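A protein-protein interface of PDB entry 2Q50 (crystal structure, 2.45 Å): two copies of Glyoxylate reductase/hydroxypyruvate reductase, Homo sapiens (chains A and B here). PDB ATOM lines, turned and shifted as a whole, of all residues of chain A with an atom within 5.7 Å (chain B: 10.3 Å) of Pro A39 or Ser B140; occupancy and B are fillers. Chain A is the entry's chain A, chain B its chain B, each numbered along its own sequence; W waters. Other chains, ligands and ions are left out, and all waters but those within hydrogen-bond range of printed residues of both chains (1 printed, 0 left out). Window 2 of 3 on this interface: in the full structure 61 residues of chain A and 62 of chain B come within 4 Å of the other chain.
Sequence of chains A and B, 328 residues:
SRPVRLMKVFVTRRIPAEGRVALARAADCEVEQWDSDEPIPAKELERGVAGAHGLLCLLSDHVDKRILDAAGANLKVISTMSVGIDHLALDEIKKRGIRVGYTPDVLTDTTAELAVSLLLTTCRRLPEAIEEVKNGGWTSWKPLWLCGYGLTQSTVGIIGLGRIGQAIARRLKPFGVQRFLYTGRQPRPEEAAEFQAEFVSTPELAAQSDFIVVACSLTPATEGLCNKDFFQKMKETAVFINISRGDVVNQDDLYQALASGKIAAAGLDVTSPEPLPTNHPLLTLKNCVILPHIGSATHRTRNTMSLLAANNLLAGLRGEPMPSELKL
The backbone carbonyl oxygen of Trp B141 lies within hydrogen-bond range of the guanidinium group of Arg A13 (2.9 Å). The side-chain hydroxyl of Thr B139 sits at hydrogen-bond distance from the side-chain carboxylate of Glu A38 (2.9 Å). NZ of Lys B142 is in salt-bridge range of OE2 of Glu A38 (2.9 Å). NH2 of Arg A13 is in hydrogen-bond range of OG of Ser B140 (3.1 Å).
The backbone carbonyl oxygen of Glu B132 sits at hydrogen-bond distance from the backbone NH of Trp B138 (3.3 Å). O of Asp A37 lies within hydrogen-bond range of NH1 of Arg A13, at 3.0 Å. N of Glu A38 sits at hydrogen-bond distance from OG of Ser A36, 3.1 Å away. NH2 of Arg A13 lies within hydrogen-bond range of OG of Ser A60, at 3.1 Å. The indole nitrogen (NE1) of Trp A34 sits at hydrogen-bond distance from the backbone carbonyl oxygen (O) of Glu A38 (3.3 Å). The guanidinium group of Arg A13 lies close to the backbone carbonyl oxygen of Glu A38, at 3.2 Å.
Among the printed residues, pairs that only touch across the chains: Arg A13 with Lys B142, Arg A13 with Pro B143, Asp A37 with Lys B142, Pro A39 with Ser B140, Ser A60 with Ser B140, Pro A275 with Trp B138, Pro A275 with Thr B139, Pro A292 with Val B133, Pro A292 with Trp B138, Pro A292 with Trp B145 and Pro A292 with Leu B146.
Ser B140 touches just these residues of chain A: Arg A13 (3.1 Å), Pro A39 (3.4 Å) and Ser A60 (3.3 Å). No residue of chain B comes within 4 Å of Ile A40. No residue of chain B comes within 4 Å of Pro A41. Of chain B, only Ser B140 (3.3 Å) comes within 4 Å of Ser A60. Of the printed residues of chain B, Pro A292 touches Val B133 (3.6 Å), Trp B138 (3.6 Å), Trp B145 (3.5 Å) and Leu B146 (3.5 Å). Of the printed residues of chain A, Thr B139 touches Glu A38 and Pro A275. Of the printed residues of chain A, Trp B141 touches Arg A13. Glu B132 touches none of the printed residues of chain A.
Along chain A the printed residues that touch a printed residue of chain B span positions 13 to 292. Of the 13 printed residues of chain B, 9 touch a printed residue of chain A. Hydrophobic or aromatic side chains of chain B that line the printed part of chain A: Val B133, Trp B138, Pro B143, Trp B145 and Leu B146. Among the printed residues, 15 pairs touch across the chains.
No position is printed for both chains.
Water W1 lies within hydrogen-bond range of O of Pro A292 and N of Lys B142.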
ATOM      1  N   ARG A  13      -1.479   3.581   5.829  1.00  0.00           N
ATOM      2  CA  ARG A  13      -2.920   3.394   5.702  1.00  0.00           C
ATOM      3  C   ARG A  13      -3.543   4.425   4.765  1.00  0.00           C
ATOM      4  O   ARG A  13      -2.918   5.425   4.422  1.00  0.00           O
ATOM      5  CB  ARG A  13      -3.560   3.520   7.096  1.00  0.00           C
ATOM      6  CG  ARG A  13      -4.990   3.025   7.205  1.00  0.00           C
ATOM      7  CD  ARG A  13      -5.036   1.518   7.405  1.00  0.00           C
ATOM      8  NE  ARG A  13      -4.706   1.130   8.770  1.00  0.00           N
ATOM      9  CZ  ARG A  13      -5.496   1.333   9.820  1.00  0.00           C
ATOM     10  NH1 ARG A  13      -6.678   1.924   9.665  1.00  0.00           N
ATOM     11  NH2 ARG A  13      -5.104   0.947  11.029  1.00  0.00           N
ATOM     12  N   TRP A  34       0.096   2.193   1.789  1.00  0.00           N
ATOM     13  CA  TRP A  34      -0.541   0.900   2.047  1.00  0.00           C
ATOM     14  C   TRP A  34      -2.009   1.017   1.621  1.00  0.00           C
ATOM     15  O   TRP A  34      -2.813   1.658   2.297  1.00  0.00           O
ATOM     16  CB  TRP A  34      -0.435   0.562   3.542  1.00  0.00           C
ATOM     17  CG  TRP A  34      -1.171  -0.681   3.999  1.00  0.00           C
ATOM     18  CD1 TRP A  34      -2.222  -0.732   4.874  1.00  0.00           C
ATOM     19  CD2 TRP A  34      -0.847  -2.045   3.688  1.00  0.00           C
ATOM     20  NE1 TRP A  34      -2.562  -2.038   5.136  1.00  0.00           N
ATOM     21  CE2 TRP A  34      -1.735  -2.864   4.421  1.00  0.00           C
ATOM     22  CE3 TRP A  34       0.112  -2.652   2.866  1.00  0.00           C
ATOM     23  CZ2 TRP A  34      -1.693  -4.266   4.357  1.00  0.00           C
ATOM     24  CZ3 TRP A  34       0.155  -4.042   2.802  1.00  0.00           C
ATOM     25  CH2 TRP A  34      -0.742  -4.833   3.545  1.00  0.00           C
ATOM     26  N   SER A  36      -5.282   0.218   1.751  1.00  0.00           N
ATOM     27  CA  SER A  36      -6.274  -0.464   2.576  1.00  0.00           C
ATOM     28  C   SER A  36      -6.653   0.332   3.823  1.00  0.00           C
ATOM     29  O   SER A  36      -5.892   1.188   4.306  1.00  0.00           O
ATOM     30  CB  SER A  36      -5.745  -1.844   3.005  1.00  0.00           C
ATOM     31  OG  SER A  36      -6.725  -2.580   3.719  1.00  0.00           O
ATOM     32  N   ASP A  37      -7.842   0.034   4.339  1.00  0.00           N
ATOM     33  CA  ASP A  37      -8.342   0.677   5.541  1.00  0.00           C
ATOM     34  C   ASP A  37      -8.105  -0.233   6.733  1.00  0.00           C
ATOM     35  O   ASP A  37      -8.312   0.165   7.878  1.00  0.00           O
ATOM     36  CB  ASP A  37      -9.831   0.996   5.403  1.00  0.00           C
ATOM     37  CG  ASP A  37     -10.090   2.100   4.406  1.00  0.00           C
ATOM     38  OD1 ASP A  37      -9.216   2.984   4.268  1.00  0.00           O
ATOM     39  OD2 ASP A  37     -11.169   2.095   3.772  1.00  0.00           O
ATOM     40  N   GLU A  38      -7.667  -1.457   6.450  1.00  0.00           N
ATOM     41  CA  GLU A  38      -7.376  -2.435   7.492  1.00  0.00           C
ATOM     42  C   GLU A  38      -5.966  -2.172   8.002  1.00  0.00           C
ATOM     43  O   GLU A  38      -5.116  -1.669   7.262  1.00  0.00           O
ATOM     44  CB  GLU A  38      -7.443  -3.863   6.937  1.00  0.00           C
ATOM     45  CG  GLU A  38      -8.792  -4.258   6.373  1.00  0.00           C
ATOM     46  CD  GLU A  38      -9.909  -4.117   7.389  1.00  0.00           C
ATOM     47  OE1 GLU A  38      -9.783  -4.689   8.493  1.00  0.00           O
ATOM     48  OE2 GLU A  38     -10.915  -3.442   7.082  1.00  0.00           O
ATOM     49  N   PRO A  39      -5.695  -2.501   9.273  1.00  0.00           N
ATOM     50  CA  PRO A  39      -4.350  -2.274   9.815  1.00  0.00           C
ATOM     51  C   PRO A  39      -3.325  -3.204   9.156  1.00  0.00           C
ATOM     52  O   PRO A  39      -3.591  -4.391   8.935  1.00  0.00           O
ATOM     53  CB  PRO A  39      -4.531  -2.548  11.310  1.00  0.00           C
ATOM     54  CG  PRO A  39      -5.616  -3.602  11.332  1.00  0.00           C
ATOM     55  CD  PRO A  39      -6.593  -3.085  10.288  1.00  0.00           C
ATOM     56  N   ILE A  40      -2.153  -2.660   8.845  1.00  0.00           N
ATOM     57  CA  ILE A  40      -1.109  -3.437   8.197  1.00  0.00           C
ATOM     58  C   ILE A  40      -0.316  -4.305   9.174  1.00  0.00           C
ATOM     59  O   ILE A  40       0.221  -3.809  10.170  1.00  0.00           O
ATOM     60  CB  ILE A  40      -0.133  -2.509   7.428  1.00  0.00           C
ATOM     61  CG1 ILE A  40       0.938  -3.345   6.731  1.00  0.00           C
ATOM     62  CG2 ILE A  40       0.499  -1.496   8.385  1.00  0.00           C
ATOM     63  CD1 ILE A  40       1.888  -2.523   5.872  1.00  0.00           C
ATOM     64  N   PRO A  41      -0.231  -5.618   8.894  1.00  0.00           N
ATOM     65  CA  PRO A  41       0.507  -6.543   9.760  1.00  0.00           C
ATOM     66  C   PRO A  41       1.910  -6.015  10.011  1.00  0.00           C
ATOM     67  O   PRO A  41       2.388  -5.148   9.287  1.00  0.00           O
ATOM     68  CB  PRO A  41       0.521  -7.837   8.952  1.00  0.00           C
ATOM     69  CG  PRO A  41      -0.778  -7.766   8.187  1.00  0.00           C
ATOM     70  CD  PRO A  41      -0.778  -6.327   7.721  1.00  0.00           C
ATOM     71  N   SER A  60      -2.751   2.379  15.471  1.00  0.00           N
ATOM     72  CA  SER A  60      -2.590   0.931  15.333  1.00  0.00           C
ATOM     73  C   SER A  60      -1.134   0.525  15.123  1.00  0.00           C
ATOM     74  O   SER A  60      -0.658  -0.437  15.717  1.00  0.00           O
ATOM     75  CB  SER A  60      -3.400   0.412  14.141  1.00  0.00           C
ATOM     76  OG  SER A  60      -2.676   0.571  12.925  1.00  0.00           O
ATOM     77  N   PRO A 275      -8.820  -4.765  18.622  1.00  0.00           N
ATOM     78  CA  PRO A 275     -10.222  -4.683  19.052  1.00  0.00           C
ATOM     79  C   PRO A 275     -10.560  -5.613  20.212  1.00  0.00           C
ATOM     80  O   PRO A 275      -9.812  -6.540  20.519  1.00  0.00           O
ATOM     81  CB  PRO A 275     -10.982  -5.053  17.787  1.00  0.00           C
ATOM     82  CG  PRO A 275     -10.103  -6.128  17.218  1.00  0.00           C
ATOM     83  CD  PRO A 275      -8.705  -5.534  17.369  1.00  0.00           C
ATOM     84  N   PRO A 292     -15.745   1.809  19.490  1.00  0.00           N
ATOM     85  CA  PRO A 292     -14.507   1.405  18.814  1.00  0.00           C
ATOM     86  C   PRO A 292     -13.467   2.515  18.642  1.00  0.00           C
ATOM     87  O   PRO A 292     -12.928   2.706  17.552  1.00  0.00           O
ATOM     88  CB  PRO A 292     -15.015   0.867  17.480  1.00  0.00           C
ATOM     89  CG  PRO A 292     -16.145   1.803  17.186  1.00  0.00           C
ATOM     90  CD  PRO A 292     -16.858   1.905  18.529  1.00  0.00           C
ATOM     91  N   GLU B 132     -21.037  -2.318  15.880  1.00  0.00           N
ATOM     92  CA  GLU B 132     -19.835  -2.786  15.200  1.00  0.00           C
ATOM     93  C   GLU B 132     -18.816  -3.471  16.120  1.00  0.00           C
ATOM     94  O   GLU B 132     -18.069  -4.349  15.690  1.00  0.00           O
ATOM     95  CB  GLU B 132     -19.177  -1.628  14.433  1.00  0.00           C
ATOM     96  CG  GLU B 132     -20.029  -1.109  13.275  1.00  0.00           C
ATOM     97  CD  GLU B 132     -20.484  -2.223  12.335  1.00  0.00           C
ATOM     98  OE1 GLU B 132     -19.657  -2.720  11.548  1.00  0.00           O
ATOM     99  OE2 GLU B 132     -21.670  -2.616  12.390  1.00  0.00           O
ATOM    100  N   VAL B 133     -18.772  -3.069  17.384  1.00  0.00           N
ATOM    101  CA  VAL B 133     -17.859  -3.695  18.324  1.00  0.00           C
ATOM    102  C   VAL B 133     -18.451  -5.067  18.620  1.00  0.00           C
ATOM    103  O   VAL B 133     -17.732  -6.043  18.832  1.00  0.00           O
ATOM    104  CB  VAL B 133     -17.767  -2.890  19.650  1.00  0.00           C
ATOM    105  CG1 VAL B 133     -17.110  -3.723  20.736  1.00  0.00           C
ATOM    106  CG2 VAL B 133     -16.981  -1.615  19.428  1.00  0.00           C
ATOM    107  N   GLY B 136     -18.321  -7.628  15.270  1.00  0.00           N
ATOM    108  CA  GLY B 136     -17.005  -7.943  14.733  1.00  0.00           C
ATOM    109  C   GLY B 136     -16.459  -7.060  13.620  1.00  0.00           C
ATOM    110  O   GLY B 136     -15.343  -7.280  13.147  1.00  0.00           O
ATOM    111  N   GLY B 137     -17.233  -6.066  13.196  1.00  0.00           N
ATOM    112  CA  GLY B 137     -16.770  -5.175  12.147  1.00  0.00           C
ATOM    113  C   GLY B 137     -15.580  -4.329  12.564  1.00  0.00           C
ATOM    114  O   GLY B 137     -14.920  -3.709  11.723  1.00  0.00           O
ATOM    115  N   TRP B 138     -15.303  -4.306  13.866  1.00  0.00           N
ATOM    116  CA  TRP B 138     -14.191  -3.531  14.416  1.00  0.00           C
ATOM    117  C   TRP B 138     -12.883  -4.310  14.312  1.00  0.00           C
ATOM    118  O   TRP B 138     -12.764  -5.409  14.845  1.00  0.00           O
ATOM    119  CB  TRP B 138     -14.487  -3.173  15.886  1.00  0.00           C
ATOM    120  CG  TRP B 138     -13.438  -2.327  16.573  1.00  0.00           C
ATOM    121  CD1 TRP B 138     -12.565  -1.452  15.984  1.00  0.00           C
ATOM    122  CD2 TRP B 138     -13.222  -2.210  17.989  1.00  0.00           C
ATOM    123  NE1 TRP B 138     -11.827  -0.800  16.943  1.00  0.00           N
ATOM    124  CE2 TRP B 138     -12.209  -1.246  18.182  1.00  0.00           C
ATOM    125  CE3 TRP B 138     -13.790  -2.827  19.114  1.00  0.00           C
ATOM    126  CZ2 TRP B 138     -11.751  -0.883  19.455  1.00  0.00           C
ATOM    127  CZ3 TRP B 138     -13.335  -2.465  20.376  1.00  0.00           C
ATOM    128  CH2 TRP B 138     -12.325  -1.501  20.535  1.00  0.00           C
ATOM    129  N   THR B 139     -11.903  -3.737  13.625  1.00  0.00           N
ATOM    130  CA  THR B 139     -10.615  -4.409  13.455  1.00  0.00           C
ATOM    131  C   THR B 139      -9.438  -3.538  13.876  1.00  0.00           C
ATOM    132  O   THR B 139      -8.369  -4.040  14.214  1.00  0.00           O
ATOM    133  CB  THR B 139     -10.411  -4.865  11.981  1.00  0.00           C
ATOM    134  OG1 THR B 139     -10.533  -3.740  11.091  1.00  0.00           O
ATOM    135  CG2 THR B 139     -11.450  -5.912  11.611  1.00  0.00           C
ATOM    136  N   SER B 140      -9.643  -2.228  13.865  1.00  0.00           N
ATOM    137  CA  SER B 140      -8.588  -1.302  14.252  1.00  0.00           C
ATOM    138  C   SER B 140      -9.046   0.142  14.204  1.00  0.00           C
ATOM    139  O   SER B 140     -10.146   0.444  13.752  1.00  0.00           O
ATOM    140  CB  SER B 140      -7.378  -1.465  13.332  1.00  0.00           C
ATOM    141  OG  SER B 140      -6.519  -0.342  13.428  1.00  0.00           O
ATOM    142  N   TRP B 141      -8.193   1.038  14.679  1.00  0.00           N
ATOM    143  CA  TRP B 141      -8.515   2.453  14.634  1.00  0.00           C
ATOM    144  C   TRP B 141      -8.574   2.767  13.142  1.00  0.00           C
ATOM    145  O   TRP B 141      -7.649   2.439  12.402  1.00  0.00           O
ATOM    146  CB  TRP B 141      -7.412   3.280  15.290  1.00  0.00           C
ATOM    147  CG  TRP B 141      -7.759   4.718  15.398  1.00  0.00           C
ATOM    148  CD1 TRP B 141      -8.453   5.322  16.410  1.00  0.00           C
ATOM    149  CD2 TRP B 141      -7.455   5.745  14.450  1.00  0.00           C
ATOM    150  NE1 TRP B 141      -8.593   6.663  16.154  1.00  0.00           N
ATOM    151  CE2 TRP B 141      -7.990   6.953  14.957  1.00  0.00           C
ATOM    152  CE3 TRP B 141      -6.783   5.765  13.219  1.00  0.00           C
ATOM    153  CZ2 TRP B 141      -7.872   8.168  14.277  1.00  0.00           C
ATOM    154  CZ3 TRP B 141      -6.668   6.971  12.540  1.00  0.00           C
ATOM    155  CH2 TRP B 141      -7.209   8.158  13.072  1.00  0.00           C
ATOM    156  N   LYS B 142      -9.664   3.381  12.699  1.00  0.00           N
ATOM    157  CA  LYS B 142      -9.822   3.718  11.293  1.00  0.00           C
ATOM    158  C   LYS B 142     -10.150   5.194  11.129  1.00  0.00           C
ATOM    159  O   LYS B 142     -11.128   5.687  11.684  1.00  0.00           O
ATOM    160  CB  LYS B 142     -10.920   2.861  10.673  1.00  0.00           C
ATOM    161  CG  LYS B 142     -10.568   1.386  10.554  1.00  0.00           C
ATOM    162  CD  LYS B 142     -11.639   0.650   9.762  1.00  0.00           C
ATOM    163  CE  LYS B 142     -11.198  -0.753   9.408  1.00  0.00           C
ATOM    164  NZ  LYS B 142     -12.287  -1.508   8.737  1.00  0.00           N
ATOM    165  N   PRO B 143      -9.325   5.917  10.351  1.00  0.00           N
ATOM    166  CA  PRO B 143      -9.455   7.352  10.069  1.00  0.00           C
ATOM    167  C   PRO B 143     -10.665   7.854   9.286  1.00  0.00           C
ATOM    168  O   PRO B 143     -11.039   9.021   9.415  1.00  0.00           O
ATOM    169  CB  PRO B 143      -8.145   7.682   9.370  1.00  0.00           C
ATOM    170  CG  PRO B 143      -7.802   6.387   8.670  1.00  0.00           C
ATOM    171  CD  PRO B 143      -8.114   5.362   9.719  1.00  0.00           C
ATOM    172  N   LEU B 144     -11.291   7.004   8.481  1.00  0.00           N
ATOM    173  CA  LEU B 144     -12.449   7.458   7.707  1.00  0.00           C
ATOM    174  C   LEU B 144     -13.710   6.753   8.182  1.00  0.00           C
ATOM    175  O   LEU B 144     -14.786   6.924   7.622  1.00  0.00           O
ATOM    176  CB  LEU B 144     -12.234   7.148   6.229  1.00  0.00           C
ATOM    177  CG  LEU B 144     -10.816   7.363   5.701  1.00  0.00           C
ATOM    178  CD1 LEU B 144     -10.730   6.891   4.254  1.00  0.00           C
ATOM    179  CD2 LEU B 144     -10.444   8.824   5.828  1.00  0.00           C
ATOM    180  N   TRP B 145     -13.552   5.981   9.249  1.00  0.00           N
ATOM    181  CA  TRP B 145     -14.607   5.168   9.823  1.00  0.00           C
ATOM    182  C   TRP B 145     -15.451   5.810  10.927  1.00  0.00           C
ATOM    183  O   TRP B 145     -14.934   6.426  11.862  1.00  0.00           O
ATOM    184  CB  TRP B 145     -13.952   3.892  10.338  1.00  0.00           C
ATOM    185  CG  TRP B 145     -14.867   2.794  10.716  1.00  0.00           C
ATOM    186  CD1 TRP B 145     -15.837   2.234   9.945  1.00  0.00           C
ATOM    187  CD2 TRP B 145     -14.817   2.029  11.923  1.00  0.00           C
ATOM    188  NE1 TRP B 145     -16.389   1.159  10.591  1.00  0.00           N
ATOM    189  CE2 TRP B 145     -15.779   1.012  11.809  1.00  0.00           C
ATOM    190  CE3 TRP B 145     -14.043   2.104  13.090  1.00  0.00           C
ATOM    191  CZ2 TRP B 145     -15.996   0.072  12.817  1.00  0.00           C
ATOM    192  CZ3 TRP B 145     -14.253   1.176  14.090  1.00  0.00           C
ATOM    193  CH2 TRP B 145     -15.224   0.169  13.949  1.00  0.00           C
ATOM    194  N   LEU B 146     -16.764   5.637  10.803  1.00  0.00           N
ATOM    195  CA  LEU B 146     -17.734   6.153  11.770  1.00  0.00           C
ATOM    196  C   LEU B 146     -17.704   7.657  12.013  1.00  0.00           C
ATOM    197  O   LEU B 146     -18.054   8.108  13.098  1.00  0.00           O
ATOM    198  CB  LEU B 146     -17.575   5.415  13.106  1.00  0.00           C
ATOM    199  CG  LEU B 146     -18.164   4.000  13.143  1.00  0.00           C
ATOM    200  CD1 LEU B 146     -17.686   3.251  14.379  1.00  0.00           C
ATOM    201  CD2 LEU B 146     -19.688   4.093  13.112  1.00  0.00           C
HETATM  202  O   HOH W   1     -11.715   4.270  15.073  1.00  0.00           O
